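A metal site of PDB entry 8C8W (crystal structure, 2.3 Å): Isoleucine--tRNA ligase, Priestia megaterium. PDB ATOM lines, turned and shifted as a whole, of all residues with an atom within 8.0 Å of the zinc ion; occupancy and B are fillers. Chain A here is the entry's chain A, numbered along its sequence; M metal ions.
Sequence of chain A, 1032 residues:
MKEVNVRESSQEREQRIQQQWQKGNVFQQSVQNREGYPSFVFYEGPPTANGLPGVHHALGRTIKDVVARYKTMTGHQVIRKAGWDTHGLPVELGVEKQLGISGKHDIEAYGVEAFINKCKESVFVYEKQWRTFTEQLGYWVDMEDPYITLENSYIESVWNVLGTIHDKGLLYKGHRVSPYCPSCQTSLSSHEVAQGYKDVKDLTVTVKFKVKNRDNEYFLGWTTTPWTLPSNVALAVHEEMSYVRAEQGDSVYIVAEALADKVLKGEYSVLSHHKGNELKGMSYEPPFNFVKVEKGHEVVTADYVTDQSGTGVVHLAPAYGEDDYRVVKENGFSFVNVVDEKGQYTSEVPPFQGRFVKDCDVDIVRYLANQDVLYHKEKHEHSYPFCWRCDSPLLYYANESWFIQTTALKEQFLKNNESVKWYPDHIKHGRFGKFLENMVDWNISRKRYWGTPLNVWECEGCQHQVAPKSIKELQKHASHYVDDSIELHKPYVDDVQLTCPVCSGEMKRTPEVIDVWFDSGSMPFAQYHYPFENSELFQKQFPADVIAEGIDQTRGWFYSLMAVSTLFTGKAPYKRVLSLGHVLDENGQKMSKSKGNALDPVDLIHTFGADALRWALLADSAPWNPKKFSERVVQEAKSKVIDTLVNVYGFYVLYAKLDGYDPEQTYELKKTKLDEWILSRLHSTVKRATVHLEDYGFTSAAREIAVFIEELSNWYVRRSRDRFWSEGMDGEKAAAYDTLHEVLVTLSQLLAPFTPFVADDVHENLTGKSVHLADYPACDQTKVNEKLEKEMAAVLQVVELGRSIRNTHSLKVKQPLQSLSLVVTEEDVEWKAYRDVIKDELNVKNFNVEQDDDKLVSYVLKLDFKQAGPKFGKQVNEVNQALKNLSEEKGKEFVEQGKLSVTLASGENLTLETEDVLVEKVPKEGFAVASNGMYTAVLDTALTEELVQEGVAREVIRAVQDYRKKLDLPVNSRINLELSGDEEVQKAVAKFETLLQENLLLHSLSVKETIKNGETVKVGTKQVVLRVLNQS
SG of Cys 387 sits close to N of Arg 389, at 3.5 Å.
N of Cys 387 lies within hydrogen-bond range of O of Ser 392, at 2.7 Å.
The backbone NH (N) of Cys 181 lies within hydrogen-bond range of the backbone carbonyl oxygen (O) of Thr 186, 3.1 Å away.
SG of Cys 390 lies close to N of Ser 392 (3.6 Å).
O of Cys 184 lies within hydrogen-bond range of NH1 of Arg 448 (2.8 Å).
The side-chain sulfur of Cys 181 sits close to the backbone NH of Ser 183 (3.5 Å).
Along chain A the residues within 4 Å of the zinc ion span positions 181 to 390.
The nearest printed residue that does not touch the zinc ion is Ser 183 (4.6 Å).
The zinc ion is bound by SG of Cys 181 (2.3 Å).
The zinc ion is bound by the side-chain sulfur (SG) of Cys 390 (2.3 Å).
SG of Cys 387 binds the zinc ion (2.3 Å).
SG of Cys 184 is bound to the zinc ion, 2.3 Å away.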
ATOM      1  N   LEU A  89     -18.806  19.828 -19.454  1.00  0.00           N
ATOM      2  CA  LEU A  89     -18.753  18.416 -19.075  1.00  0.00           C
ATOM      3  C   LEU A  89     -17.768  18.110 -17.960  1.00  0.00           C
ATOM      4  O   LEU A  89     -18.103  17.289 -17.084  1.00  0.00           O
ATOM      5  CB  LEU A  89     -18.439  17.560 -20.303  1.00  0.00           C
ATOM      6  CG  LEU A  89     -19.545  17.404 -21.355  1.00  0.00           C
ATOM      7  CD1 LEU A  89     -18.954  16.925 -22.674  1.00  0.00           C
ATOM      8  CD2 LEU A  89     -20.606  16.433 -20.864  1.00  0.00           C
ATOM      9  N   LEU A  93     -20.240  16.138 -15.171  1.00  0.00           N
ATOM     10  CA  LEU A  93     -20.172  14.707 -14.903  1.00  0.00           C
ATOM     11  C   LEU A  93     -19.802  14.421 -13.462  1.00  0.00           C
ATOM     12  O   LEU A  93     -20.345  13.499 -12.838  1.00  0.00           O
ATOM     13  CB  LEU A  93     -19.184  14.046 -15.868  1.00  0.00           C
ATOM     14  CG  LEU A  93     -19.577  14.086 -17.342  1.00  0.00           C
ATOM     15  CD1 LEU A  93     -18.619  13.257 -18.187  1.00  0.00           C
ATOM     16  CD2 LEU A  93     -21.008  13.597 -17.537  1.00  0.00           C
ATOM     17  N   TYR A 180     -19.663  11.942 -31.728  1.00  0.00           N
ATOM     18  CA  TYR A 180     -20.777  12.008 -30.790  1.00  0.00           C
ATOM     19  C   TYR A 180     -20.532  11.036 -29.645  1.00  0.00           C
ATOM     20  O   TYR A 180     -20.145   9.887 -29.878  1.00  0.00           O
ATOM     21  CB  TYR A 180     -22.102  11.686 -31.504  1.00  0.00           C
ATOM     22  CG  TYR A 180     -23.331  11.759 -30.634  1.00  0.00           C
ATOM     23  CD1 TYR A 180     -23.996  12.965 -30.428  1.00  0.00           C
ATOM     24  CD2 TYR A 180     -23.838  10.614 -30.020  1.00  0.00           C
ATOM     25  CE1 TYR A 180     -25.129  13.032 -29.632  1.00  0.00           C
ATOM     26  CE2 TYR A 180     -24.971  10.674 -29.231  1.00  0.00           C
ATOM     27  CZ  TYR A 180     -25.606  11.887 -29.035  1.00  0.00           C
ATOM     28  OH  TYR A 180     -26.728  11.933 -28.243  1.00  0.00           O
ATOM     29  N   CYS A 181     -20.776  11.500 -28.425  1.00  0.00           N
ATOM     30  CA  CYS A 181     -20.648  10.637 -27.252  1.00  0.00           C
ATOM     31  C   CYS A 181     -22.011  10.120 -26.855  1.00  0.00           C
ATOM     32  O   CYS A 181     -22.872  10.915 -26.433  1.00  0.00           O
ATOM     33  CB  CYS A 181     -20.003  11.379 -26.089  1.00  0.00           C
ATOM     34  SG  CYS A 181     -19.925  10.369 -24.598  1.00  0.00           S
ATOM     35  N   PRO A 182     -22.277   8.813 -26.964  1.00  0.00           N
ATOM     36  CA  PRO A 182     -23.600   8.288 -26.588  1.00  0.00           C
ATOM     37  C   PRO A 182     -23.887   8.349 -25.103  1.00  0.00           C
ATOM     38  O   PRO A 182     -25.067   8.308 -24.717  1.00  0.00           O
ATOM     39  CB  PRO A 182     -23.557   6.836 -27.087  1.00  0.00           C
ATOM     40  CG  PRO A 182     -22.105   6.492 -27.110  1.00  0.00           C
ATOM     41  CD  PRO A 182     -21.381   7.752 -27.474  1.00  0.00           C
ATOM     42  N   SER A 183     -22.869   8.445 -24.253  1.00  0.00           N
ATOM     43  CA  SER A 183     -23.101   8.539 -22.812  1.00  0.00           C
ATOM     44  C   SER A 183     -23.400   9.981 -22.401  1.00  0.00           C
ATOM     45  O   SER A 183     -24.428  10.251 -21.771  1.00  0.00           O
ATOM     46  CB  SER A 183     -21.907   8.002 -22.037  1.00  0.00           C
ATOM     47  OG  SER A 183     -22.122   8.095 -20.648  1.00  0.00           O
ATOM     48  N   CYS A 184     -22.498  10.907 -22.746  1.00  0.00           N
ATOM     49  CA  CYS A 184     -22.754  12.325 -22.490  1.00  0.00           C
ATOM     50  C   CYS A 184     -23.893  12.865 -23.354  1.00  0.00           C
ATOM     51  O   CYS A 184     -24.448  13.924 -23.018  1.00  0.00           O
ATOM     52  CB  CYS A 184     -21.476  13.137 -22.738  1.00  0.00           C
ATOM     53  SG  CYS A 184     -20.134  12.808 -21.570  1.00  0.00           S
ATOM     54  N   GLN A 185     -24.227  12.180 -24.442  1.00  0.00           N
ATOM     55  CA  GLN A 185     -25.370  12.511 -25.302  1.00  0.00           C
ATOM     56  C   GLN A 185     -25.224  13.906 -25.911  1.00  0.00           C
ATOM     57  O   GLN A 185     -26.130  14.734 -25.874  1.00  0.00           O
ATOM     58  CB  GLN A 185     -26.701  12.380 -24.547  1.00  0.00           C
ATOM     59  CG  GLN A 185     -27.027  10.955 -24.134  1.00  0.00           C
ATOM     60  CD  GLN A 185     -28.351  10.850 -23.398  1.00  0.00           C
ATOM     61  OE1 GLN A 185     -29.339  11.500 -23.778  1.00  0.00           O
ATOM     62  NE2 GLN A 185     -28.396  10.043 -22.351  1.00  0.00           N
ATOM     63  N   THR A 186     -24.043  14.172 -26.483  1.00  0.00           N
ATOM     64  CA  THR A 186     -23.791  15.435 -27.157  1.00  0.00           C
ATOM     65  C   THR A 186     -22.679  15.224 -28.169  1.00  0.00           C
ATOM     66  O   THR A 186     -21.838  14.338 -28.019  1.00  0.00           O
ATOM     67  CB  THR A 186     -23.415  16.539 -26.166  1.00  0.00           C
ATOM     68  OG1 THR A 186     -23.192  17.763 -26.875  1.00  0.00           O
ATOM     69  CG2 THR A 186     -22.154  16.166 -25.396  1.00  0.00           C
ATOM     70  N   LEU A 188     -19.201  16.431 -30.075  1.00  0.00           N
ATOM     71  CA  LEU A 188     -17.928  16.897 -29.537  1.00  0.00           C
ATOM     72  C   LEU A 188     -17.136  17.626 -30.625  1.00  0.00           C
ATOM     73  O   LEU A 188     -17.376  17.456 -31.821  1.00  0.00           O
ATOM     74  CB  LEU A 188     -17.091  15.737 -28.989  1.00  0.00           C
ATOM     75  CG  LEU A 188     -17.663  14.960 -27.800  1.00  0.00           C
ATOM     76  CD1 LEU A 188     -16.649  13.935 -27.315  1.00  0.00           C
ATOM     77  CD2 LEU A 188     -18.062  15.919 -26.674  1.00  0.00           C
ATOM     78  N   PHE A 386     -12.568   7.907 -28.272  1.00  0.00           N
ATOM     79  CA  PHE A 386     -13.325   7.744 -27.032  1.00  0.00           C
ATOM     80  C   PHE A 386     -13.544   9.111 -26.401  1.00  0.00           C
ATOM     81  O   PHE A 386     -12.777  10.047 -26.627  1.00  0.00           O
ATOM     82  CB  PHE A 386     -12.591   6.823 -26.042  1.00  0.00           C
ATOM     83  CG  PHE A 386     -12.612   5.378 -26.431  1.00  0.00           C
ATOM     84  CD1 PHE A 386     -11.811   4.901 -27.444  1.00  0.00           C
ATOM     85  CD2 PHE A 386     -13.436   4.483 -25.756  1.00  0.00           C
ATOM     86  CE1 PHE A 386     -11.830   3.570 -27.804  1.00  0.00           C
ATOM     87  CE2 PHE A 386     -13.453   3.146 -26.109  1.00  0.00           C
ATOM     88  CZ  PHE A 386     -12.655   2.689 -27.132  1.00  0.00           C
ATOM     89  N   CYS A 387     -14.611   9.220 -25.610  1.00  0.00           N
ATOM     90  CA  CYS A 387     -14.923  10.494 -24.972  1.00  0.00           C
ATOM     91  C   CYS A 387     -13.836  10.863 -23.967  1.00  0.00           C
ATOM     92  O   CYS A 387     -13.490  10.067 -23.091  1.00  0.00           O
ATOM     93  CB  CYS A 387     -16.285  10.440 -24.295  1.00  0.00           C
ATOM     94  SG  CYS A 387     -16.702  11.966 -23.411  1.00  0.00           S
ATOM     95  N   TRP A 388     -13.336  12.099 -24.079  1.00  0.00           N
ATOM     96  CA  TRP A 388     -12.225  12.534 -23.239  1.00  0.00           C
ATOM     97  C   TRP A 388     -12.634  12.731 -21.781  1.00  0.00           C
ATOM     98  O   TRP A 388     -11.766  12.943 -20.932  1.00  0.00           O
ATOM     99  CB  TRP A 388     -11.615  13.830 -23.785  1.00  0.00           C
ATOM    100  CG  TRP A 388     -12.506  15.034 -23.677  1.00  0.00           C
ATOM    101  CD1 TRP A 388     -13.730  15.210 -24.245  1.00  0.00           C
ATOM    102  CD2 TRP A 388     -12.225  16.241 -22.945  1.00  0.00           C
ATOM    103  NE1 TRP A 388     -14.238  16.439 -23.906  1.00  0.00           N
ATOM    104  CE2 TRP A 388     -13.336  17.092 -23.112  1.00  0.00           C
ATOM    105  CE3 TRP A 388     -11.148  16.682 -22.169  1.00  0.00           C
ATOM    106  CZ2 TRP A 388     -13.401  18.361 -22.542  1.00  0.00           C
ATOM    107  CZ3 TRP A 388     -11.211  17.937 -21.597  1.00  0.00           C
ATOM    108  CH2 TRP A 388     -12.332  18.763 -21.781  1.00  0.00           C
ATOM    109  N   ARG A 389     -13.937  12.673 -21.466  1.00  0.00           N
ATOM    110  CA  ARG A 389     -14.409  12.818 -20.096  1.00  0.00           C
ATOM    111  C   ARG A 389     -14.893  11.500 -19.494  1.00  0.00           C
ATOM    112  O   ARG A 389     -14.446  11.121 -18.406  1.00  0.00           O
ATOM    113  CB  ARG A 389     -15.531  13.866 -20.020  1.00  0.00           C
ATOM    114  CG  ARG A 389     -15.136  15.247 -20.507  1.00  0.00           C
ATOM    115  CD  ARG A 389     -13.789  15.682 -19.937  1.00  0.00           C
ATOM    116  NE  ARG A 389     -13.773  15.700 -18.479  1.00  0.00           N
ATOM    117  CZ  ARG A 389     -12.722  16.059 -17.745  1.00  0.00           C
ATOM    118  NH1 ARG A 389     -11.588  16.433 -18.299  1.00  0.00           N
ATOM    119  NH2 ARG A 389     -12.831  16.042 -16.418  1.00  0.00           N
ATOM    120  N   CYS A 390     -15.803  10.798 -20.163  1.00  0.00           N
ATOM    121  CA  CYS A 390     -16.419   9.598 -19.599  1.00  0.00           C
ATOM    122  C   CYS A 390     -15.868   8.294 -20.163  1.00  0.00           C
ATOM    123  O   CYS A 390     -16.355   7.222 -19.795  1.00  0.00           O
ATOM    124  CB  CYS A 390     -17.942   9.648 -19.806  1.00  0.00           C
ATOM    125  SG  CYS A 390     -18.474   9.360 -21.499  1.00  0.00           S
ATOM    126  N   ASP A 391     -14.882   8.354 -21.062  1.00  0.00           N
ATOM    127  CA  ASP A 391     -14.204   7.202 -21.646  1.00  0.00           C
ATOM    128  C   ASP A 391     -15.125   6.280 -22.439  1.00  0.00           C
ATOM    129  O   ASP A 391     -14.728   5.165 -22.808  1.00  0.00           O
ATOM    130  CB  ASP A 391     -13.454   6.389 -20.583  1.00  0.00           C
ATOM    131  CG  ASP A 391     -12.032   6.882 -20.359  1.00  0.00           C
ATOM    132  OD1 ASP A 391     -11.616   7.829 -21.061  1.00  0.00           O
ATOM    133  OD2 ASP A 391     -11.333   6.325 -19.494  1.00  0.00           O
ATOM    134  N   SER A 392     -16.351   6.710 -22.724  1.00  0.00           N
ATOM    135  CA  SER A 392     -17.206   5.918 -23.594  1.00  0.00           C
ATOM    136  C   SER A 392     -16.694   5.979 -25.033  1.00  0.00           C
ATOM    137  O   SER A 392     -16.157   7.009 -25.461  1.00  0.00           O
ATOM    138  CB  SER A 392     -18.650   6.434 -23.539  1.00  0.00           C
ATOM    139  OG  SER A 392     -19.380   6.020 -24.688  1.00  0.00           O
ATOM    140  N   PRO A 393     -16.836   4.895 -25.795  1.00  0.00           N
ATOM    141  CA  PRO A 393     -16.525   4.963 -27.219  1.00  0.00           C
ATOM    142  C   PRO A 393     -17.439   5.965 -27.914  1.00  0.00           C
ATOM    143  O   PRO A 393     -18.624   6.080 -27.579  1.00  0.00           O
ATOM    144  CB  PRO A 393     -16.775   3.529 -27.708  1.00  0.00           C
ATOM    145  CG  PRO A 393     -17.736   2.961 -26.722  1.00  0.00           C
ATOM    146  CD  PRO A 393     -17.362   3.571 -25.399  1.00  0.00           C
ATOM    147  N   LEU A 394     -16.871   6.700 -28.864  1.00  0.00           N
ATOM    148  CA  LEU A 394     -17.645   7.667 -29.623  1.00  0.00           C
ATOM    149  C   LEU A 394     -18.290   7.018 -30.833  1.00  0.00           C
ATOM    150  O   LEU A 394     -17.873   5.944 -31.297  1.00  0.00           O
ATOM    151  CB  LEU A 394     -16.769   8.838 -30.078  1.00  0.00           C
ATOM    152  CG  LEU A 394     -16.067   9.682 -29.009  1.00  0.00           C
ATOM    153  CD1 LEU A 394     -15.408  10.889 -29.670  1.00  0.00           C
ATOM    154  CD2 LEU A 394     -17.051  10.110 -27.936  1.00  0.00           C
ATOM    155  N   ARG A 448     -26.446  20.194 -23.202  1.00  0.00           N
ATOM    156  CA  ARG A 448     -26.248  20.051 -21.765  1.00  0.00           C
ATOM    157  C   ARG A 448     -26.890  21.237 -21.052  1.00  0.00           C
ATOM    158  O   ARG A 448     -27.641  22.009 -21.668  1.00  0.00           O
ATOM    159  CB  ARG A 448     -24.762  19.952 -21.418  1.00  0.00           C
ATOM    160  CG  ARG A 448     -24.038  18.853 -22.166  1.00  0.00           C
ATOM    161  CD  ARG A 448     -24.517  17.477 -21.726  1.00  0.00           C
ATOM    162  NE  ARG A 448     -24.202  17.221 -20.330  1.00  0.00           N
ATOM    163  CZ  ARG A 448     -24.295  16.029 -19.748  1.00  0.00           C
ATOM    164  NH1 ARG A 448     -24.685  14.966 -20.430  1.00  0.00           N
ATOM    165  NH2 ARG A 448     -23.967  15.904 -18.472  1.00  0.00           N
HETATM  166 ZN    ZN M   1     -18.830  11.274 -22.766  1.00  0.00          ZN
